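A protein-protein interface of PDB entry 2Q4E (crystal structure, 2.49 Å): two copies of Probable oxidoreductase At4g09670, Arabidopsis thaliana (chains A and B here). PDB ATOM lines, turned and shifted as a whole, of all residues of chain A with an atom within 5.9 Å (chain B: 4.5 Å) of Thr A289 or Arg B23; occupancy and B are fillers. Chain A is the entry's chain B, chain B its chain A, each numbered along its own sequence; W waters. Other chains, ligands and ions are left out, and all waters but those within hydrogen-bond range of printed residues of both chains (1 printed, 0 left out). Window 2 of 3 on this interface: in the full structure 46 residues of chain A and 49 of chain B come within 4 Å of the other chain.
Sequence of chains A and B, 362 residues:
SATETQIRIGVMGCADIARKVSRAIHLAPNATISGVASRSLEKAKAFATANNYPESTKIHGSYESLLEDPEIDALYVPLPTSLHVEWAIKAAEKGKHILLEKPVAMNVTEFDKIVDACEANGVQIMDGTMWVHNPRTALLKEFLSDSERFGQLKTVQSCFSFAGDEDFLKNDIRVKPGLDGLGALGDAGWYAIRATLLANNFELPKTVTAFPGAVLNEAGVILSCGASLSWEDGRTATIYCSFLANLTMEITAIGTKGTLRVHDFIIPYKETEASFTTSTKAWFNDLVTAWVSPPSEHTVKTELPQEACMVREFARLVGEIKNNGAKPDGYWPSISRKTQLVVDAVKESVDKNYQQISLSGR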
ATOM      1  N   PHE A 284     -24.892  27.747  26.275  1.00  0.00           N
ATOM      2  CA  PHE A 284     -23.523  27.377  26.616  1.00  0.00           C
ATOM      3  C   PHE A 284     -22.588  27.611  25.426  1.00  0.00           C
ATOM      4  O   PHE A 284     -23.042  27.817  24.293  1.00  0.00           O
ATOM      5  CB  PHE A 284     -23.473  25.891  26.981  1.00  0.00           C
ATOM      6  CG  PHE A 284     -24.523  25.466  27.972  1.00  0.00           C
ATOM      7  CD1 PHE A 284     -24.431  25.834  29.309  1.00  0.00           C
ATOM      8  CD2 PHE A 284     -25.589  24.664  27.572  1.00  0.00           C
ATOM      9  CE1 PHE A 284     -25.376  25.407  30.232  1.00  0.00           C
ATOM     10  CE2 PHE A 284     -26.548  24.228  28.494  1.00  0.00           C
ATOM     11  CZ  PHE A 284     -26.439  24.600  29.825  1.00  0.00           C
ATOM     12  N   ASN A 285     -21.284  27.585  25.689  1.00  0.00           N
ATOM     13  CA  ASN A 285     -20.294  27.739  24.630  1.00  0.00           C
ATOM     14  C   ASN A 285     -20.247  26.385  23.921  1.00  0.00           C
ATOM     15  O   ASN A 285     -20.579  25.364  24.518  1.00  0.00           O
ATOM     16  CB  ASN A 285     -18.919  28.067  25.222  1.00  0.00           C
ATOM     17  CG  ASN A 285     -18.568  27.176  26.398  1.00  0.00           C
ATOM     18  OD1 ASN A 285     -19.182  26.121  26.602  1.00  0.00           O
ATOM     19  ND2 ASN A 285     -17.574  27.591  27.178  1.00  0.00           N
ATOM     20  N   LEU A 287     -18.637  23.839  23.580  1.00  0.00           N
ATOM     21  CA  LEU A 287     -18.311  22.627  24.326  1.00  0.00           C
ATOM     22  C   LEU A 287     -19.049  22.442  25.661  1.00  0.00           C
ATOM     23  O   LEU A 287     -18.856  21.435  26.354  1.00  0.00           O
ATOM     24  CB  LEU A 287     -16.796  22.581  24.539  1.00  0.00           C
ATOM     25  CG  LEU A 287     -16.120  21.215  24.702  1.00  0.00           C
ATOM     26  CD1 LEU A 287     -16.574  20.247  23.615  1.00  0.00           C
ATOM     27  CD2 LEU A 287     -14.615  21.410  24.639  1.00  0.00           C
ATOM     28  N   VAL A 288     -19.901  23.406  26.010  1.00  0.00           N
ATOM     29  CA  VAL A 288     -20.680  23.370  27.253  1.00  0.00           C
ATOM     30  C   VAL A 288     -19.801  23.353  28.513  1.00  0.00           C
ATOM     31  O   VAL A 288     -20.072  22.615  29.457  1.00  0.00           O
ATOM     32  CB  VAL A 288     -21.630  22.138  27.280  1.00  0.00           C
ATOM     33  CG1 VAL A 288     -22.663  22.291  28.383  1.00  0.00           C
ATOM     34  CG2 VAL A 288     -22.309  21.968  25.922  1.00  0.00           C
ATOM     35  N   THR A 289     -18.744  24.164  28.519  1.00  0.00           N
ATOM     36  CA  THR A 289     -17.862  24.247  29.677  1.00  0.00           C
ATOM     37  C   THR A 289     -18.148  25.535  30.441  1.00  0.00           C
ATOM     38  O   THR A 289     -17.498  25.833  31.447  1.00  0.00           O
ATOM     39  CB  THR A 289     -16.342  24.211  29.275  1.00  0.00           C
ATOM     40  OG1 THR A 289     -16.061  25.217  28.291  1.00  0.00           O
ATOM     41  CG2 THR A 289     -15.963  22.835  28.734  1.00  0.00           C
ATOM     42  N   ALA A 290     -19.135  26.286  29.952  1.00  0.00           N
ATOM     43  CA  ALA A 290     -19.544  27.548  30.561  1.00  0.00           C
ATOM     44  C   ALA A 290     -20.778  28.139  29.865  1.00  0.00           C
ATOM     45  O   ALA A 290     -21.075  27.785  28.719  1.00  0.00           O
ATOM     46  CB  ALA A 290     -18.386  28.551  30.494  1.00  0.00           C
ATOM     47  N   TRP A 291     -21.502  29.012  30.571  1.00  0.00           N
ATOM     48  CA  TRP A 291     -22.669  29.700  30.007  1.00  0.00           C
ATOM     49  C   TRP A 291     -22.076  30.791  29.125  1.00  0.00           C
ATOM     50  O   TRP A 291     -21.060  31.383  29.482  1.00  0.00           O
ATOM     51  CB  TRP A 291     -23.491  30.412  31.091  1.00  0.00           C
ATOM     52  CG  TRP A 291     -24.357  29.549  31.952  1.00  0.00           C
ATOM     53  CD1 TRP A 291     -23.991  28.408  32.607  1.00  0.00           C
ATOM     54  CD2 TRP A 291     -25.724  29.798  32.311  1.00  0.00           C
ATOM     55  NE1 TRP A 291     -25.045  27.933  33.350  1.00  0.00           N
ATOM     56  CE2 TRP A 291     -26.120  28.766  33.189  1.00  0.00           C
ATOM     57  CE3 TRP A 291     -26.652  30.794  31.977  1.00  0.00           C
ATOM     58  CZ2 TRP A 291     -27.412  28.699  33.742  1.00  0.00           C
ATOM     59  CZ3 TRP A 291     -27.943  30.728  32.527  1.00  0.00           C
ATOM     60  CH2 TRP A 291     -28.306  29.685  33.401  1.00  0.00           C
ATOM     61  N   ARG B  19     -17.180  14.906  22.963  1.00  0.00           N
ATOM     62  CA  ARG B  19     -16.192  15.948  22.699  1.00  0.00           C
ATOM     63  C   ARG B  19     -15.781  16.619  24.004  1.00  0.00           C
ATOM     64  O   ARG B  19     -14.646  17.068  24.154  1.00  0.00           O
ATOM     65  CB  ARG B  19     -16.747  16.997  21.726  1.00  0.00           C
ATOM     66  CG  ARG B  19     -17.078  16.461  20.335  1.00  0.00           C
ATOM     67  CD  ARG B  19     -17.376  17.588  19.349  1.00  0.00           C
ATOM     68  NE  ARG B  19     -18.547  18.374  19.731  1.00  0.00           N
ATOM     69  CZ  ARG B  19     -18.520  19.674  20.020  1.00  0.00           C
ATOM     70  NH1 ARG B  19     -17.375  20.344  19.971  1.00  0.00           N
ATOM     71  NH2 ARG B  19     -19.637  20.308  20.348  1.00  0.00           N
ATOM     72  N   LYS B  20     -16.712  16.682  24.949  1.00  0.00           N
ATOM     73  CA  LYS B  20     -16.439  17.289  26.248  1.00  0.00           C
ATOM     74  C   LYS B  20     -15.763  16.284  27.177  1.00  0.00           C
ATOM     75  O   LYS B  20     -14.825  16.623  27.902  1.00  0.00           O
ATOM     76  CB  LYS B  20     -17.745  17.769  26.885  1.00  0.00           C
ATOM     77  CG  LYS B  20     -17.577  18.430  28.236  1.00  0.00           C
ATOM     78  CD  LYS B  20     -18.926  18.717  28.881  1.00  0.00           C
ATOM     79  CE  LYS B  20     -18.753  19.354  30.252  1.00  0.00           C
ATOM     80  NZ  LYS B  20     -20.056  19.549  30.932  1.00  0.00           N
ATOM     81  N   VAL B  21     -16.233  15.041  27.156  1.00  0.00           N
ATOM     82  CA  VAL B  21     -15.647  14.027  28.023  1.00  0.00           C
ATOM     83  C   VAL B  21     -14.207  13.662  27.653  1.00  0.00           C
ATOM     84  O   VAL B  21     -13.400  13.367  28.537  1.00  0.00           O
ATOM     85  CB  VAL B  21     -16.517  12.761  28.060  1.00  0.00           C
ATOM     86  CG1 VAL B  21     -15.842  11.689  28.904  1.00  0.00           C
ATOM     87  CG2 VAL B  21     -17.887  13.105  28.645  1.00  0.00           C
ATOM     88  N   SER B  22     -13.873  13.685  26.365  1.00  0.00           N
ATOM     89  CA  SER B  22     -12.506  13.375  25.957  1.00  0.00           C
ATOM     90  C   SER B  22     -11.592  14.329  26.721  1.00  0.00           C
ATOM     91  O   SER B  22     -10.505  13.943  27.169  1.00  0.00           O
ATOM     92  CB  SER B  22     -12.334  13.553  24.450  1.00  0.00           C
ATOM     93  OG  SER B  22     -13.112  12.608  23.749  1.00  0.00           O
ATOM     94  N   ARG B  23     -12.055  15.571  26.869  1.00  0.00           N
ATOM     95  CA  ARG B  23     -11.330  16.597  27.621  1.00  0.00           C
ATOM     96  C   ARG B  23     -11.198  16.099  29.065  1.00  0.00           C
ATOM     97  O   ARG B  23     -10.108  16.117  29.640  1.00  0.00           O
ATOM     98  CB  ARG B  23     -12.102  17.932  27.604  1.00  0.00           C
ATOM     99  CG  ARG B  23     -11.543  19.013  28.538  1.00  0.00           C
ATOM    100  CD  ARG B  23     -10.661  20.029  27.817  1.00  0.00           C
ATOM    101  NE  ARG B  23     -11.371  21.256  27.458  1.00  0.00           N
ATOM    102  CZ  ARG B  23     -11.709  22.219  28.318  1.00  0.00           C
ATOM    103  NH1 ARG B  23     -11.406  22.113  29.606  1.00  0.00           N
ATOM    104  NH2 ARG B  23     -12.357  23.295  27.890  1.00  0.00           N
ATOM    105  N   ALA B  24     -12.315  15.660  29.646  1.00  0.00           N
ATOM    106  CA  ALA B  24     -12.310  15.147  31.016  1.00  0.00           C
ATOM    107  C   ALA B  24     -11.198  14.112  31.087  1.00  0.00           C
ATOM    108  O   ALA B  24     -10.209  14.297  31.791  1.00  0.00           O
ATOM    109  CB  ALA B  24     -13.638  14.501  31.341  1.00  0.00           C
ATOM    110  N   ILE B  25     -11.367  13.028  30.336  1.00  0.00           N
ATOM    111  CA  ILE B  25     -10.375  11.966  30.281  1.00  0.00           C
ATOM    112  C   ILE B  25      -8.974  12.570  30.169  1.00  0.00           C
ATOM    113  O   ILE B  25      -8.112  12.326  31.014  1.00  0.00           O
ATOM    114  CB  ILE B  25     -10.614  11.054  29.062  1.00  0.00           C
ATOM    115  CG1 ILE B  25     -11.965  10.348  29.199  1.00  0.00           C
ATOM    116  CG2 ILE B  25      -9.476  10.045  28.935  1.00  0.00           C
ATOM    117  CD1 ILE B  25     -12.339   9.511  28.011  1.00  0.00           C
ATOM    118  N   HIS B  26      -8.766  13.365  29.124  1.00  0.00           N
ATOM    119  CA  HIS B  26      -7.484  14.017  28.882  1.00  0.00           C
ATOM    120  C   HIS B  26      -6.945  14.659  30.161  1.00  0.00           C
ATOM    121  O   HIS B  26      -5.961  14.193  30.734  1.00  0.00           O
ATOM    122  CB  HIS B  26      -7.642  15.086  27.798  1.00  0.00           C
ATOM    123  CG  HIS B  26      -6.347  15.689  27.342  1.00  0.00           C
ATOM    124  ND1 HIS B  26      -6.293  16.800  26.529  1.00  0.00           N
ATOM    125  CD2 HIS B  26      -5.063  15.326  27.570  1.00  0.00           C
ATOM    126  CE1 HIS B  26      -5.030  17.096  26.275  1.00  0.00           C
ATOM    127  NE2 HIS B  26      -4.264  16.218  26.896  1.00  0.00           N
ATOM    128  N   LEU B  27      -7.609  15.726  30.597  1.00  0.00           N
ATOM    129  CA  LEU B  27      -7.234  16.474  31.796  1.00  0.00           C
ATOM    130  C   LEU B  27      -7.094  15.636  33.067  1.00  0.00           C
ATOM    131  O   LEU B  27      -6.467  16.070  34.035  1.00  0.00           O
ATOM    132  CB  LEU B  27      -8.245  17.595  32.036  1.00  0.00           C
ATOM    133  CG  LEU B  27      -8.320  18.649  30.926  1.00  0.00           C
ATOM    134  CD1 LEU B  27      -9.413  19.653  31.251  1.00  0.00           C
ATOM    135  CD2 LEU B  27      -6.972  19.346  30.784  1.00  0.00           C
ATOM    136  N   LYS B 270     -18.646  29.170  34.992  1.00  0.00           N
ATOM    137  CA  LYS B 270     -17.262  29.048  34.538  1.00  0.00           C
ATOM    138  C   LYS B 270     -16.692  27.780  35.164  1.00  0.00           C
ATOM    139  O   LYS B 270     -16.821  27.574  36.370  1.00  0.00           O
ATOM    140  CB  LYS B 270     -16.441  30.268  34.975  1.00  0.00           C
ATOM    141  CG  LYS B 270     -16.895  31.564  34.332  1.00  0.00           C
ATOM    142  CD  LYS B 270     -15.933  32.714  34.601  1.00  0.00           C
ATOM    143  CE  LYS B 270     -15.898  33.105  36.071  1.00  0.00           C
ATOM    144  NZ  LYS B 270     -15.023  34.292  36.307  1.00  0.00           N
ATOM    145  N   GLU B 271     -16.057  26.932  34.360  1.00  0.00           N
ATOM    146  CA  GLU B 271     -15.525  25.676  34.888  1.00  0.00           C
ATOM    147  C   GLU B 271     -14.465  25.872  35.968  1.00  0.00           C
ATOM    148  O   GLU B 271     -14.092  24.923  36.654  1.00  0.00           O
ATOM    149  CB  GLU B 271     -14.951  24.824  33.755  1.00  0.00           C
ATOM    150  CG  GLU B 271     -13.626  25.320  33.196  1.00  0.00           C
ATOM    151  CD  GLU B 271     -13.148  24.490  32.020  1.00  0.00           C
ATOM    152  OE1 GLU B 271     -12.076  24.812  31.461  1.00  0.00           O
ATOM    153  OE2 GLU B 271     -13.842  23.520  31.650  1.00  0.00           O
ATOM    154  N   PRO B 305     -11.873  20.993  35.980  1.00  0.00           N
ATOM    155  CA  PRO B 305     -13.301  20.927  35.640  1.00  0.00           C
ATOM    156  C   PRO B 305     -13.995  19.732  36.291  1.00  0.00           C
ATOM    157  O   PRO B 305     -13.341  18.761  36.663  1.00  0.00           O
ATOM    158  CB  PRO B 305     -13.289  20.831  34.114  1.00  0.00           C
ATOM    159  CG  PRO B 305     -12.052  21.566  33.735  1.00  0.00           C
ATOM    160  CD  PRO B 305     -11.053  21.077  34.757  1.00  0.00           C
ATOM    161  N   GLU B 307     -16.119  17.527  34.916  1.00  0.00           N
ATOM    162  CA  GLU B 307     -16.042  16.349  34.064  1.00  0.00           C
ATOM    163  C   GLU B 307     -14.627  15.814  34.199  1.00  0.00           C
ATOM    164  O   GLU B 307     -14.378  14.626  34.021  1.00  0.00           O
ATOM    165  CB  GLU B 307     -16.329  16.704  32.605  1.00  0.00           C
ATOM    166  CG  GLU B 307     -15.465  17.825  32.060  1.00  0.00           C
ATOM    167  CD  GLU B 307     -16.054  19.205  32.328  1.00  0.00           C
ATOM    168  OE1 GLU B 307     -16.572  19.441  33.442  1.00  0.00           O
ATOM    169  OE2 GLU B 307     -15.990  20.058  31.422  1.00  0.00           O
HETATM  170  O   HOH W   1     -18.925  25.291  33.694  1.00  0.00           O
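N of Thr A289 lies within hydrogen-bond range of OD1 of Asn A285 (2.8 Å). The backbone NH (N) of Val A288 sits at hydrogen-bond distance from the side-chain amide oxygen (OD1) of Asn A285, at 2.9 Å. NH1 of Arg B23 is in salt-bridge range of OE1 of Glu B271, 3.3 Å away.
Of the 13 printed residues of chain B, 5 touch a printed residue of chain A. Of the 7 printed residues of chain A, 3 touch a printed residue of chain B. Printed residues of chain A that touch a printed residue of chain B: Leu A287, Val A288 and Thr A289. Hydrophobic or aromatic side chains of chain A within 4 Å of the printed part of chain B: Leu A287.
Thr A289 touches three residues of chain B. Of chain A, only Thr A289 (3.7 Å) comes within 4 Å of Arg B23. Of the printed residues of chain A, Arg B19 touches Leu A287. Of the printed residues of chain B, Leu A287 touches Arg B19 and Lys B20. Printed residues of chain A within 4 Å of Glu B271: Thr A289. The nearest residue of chain B that does not touch Thr A289 is Lys B270 (4.3 Å). The nearest printed residue of chain B that does not touch Leu A287 is Arg B23 (4.3 Å).
Water W1 bridges O of Thr A289 and N of Glu B271.
No position is printed for both chains. Of the 6 pairs that touch across the chains among the printed residues, none has its exchanged pair printed and touching as well.
Among the printed residues, pairs that only touch across the chains: Leu A287 with Lys B20 (3.7 Å), Thr A289 with Arg B23 (3.7 Å), Leu A287 with Arg B19 (3.7 Å) and Thr A289 with Glu B307 (3.9 Å).
NZ of Lys B20 is in hydrogen-bond range of O of Val A288 (3.4 Å). The backbone NH (N) of Glu B271 sits at hydrogen-bond distance from the backbone carbonyl oxygen (O) of Thr A289 (3.4 Å).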
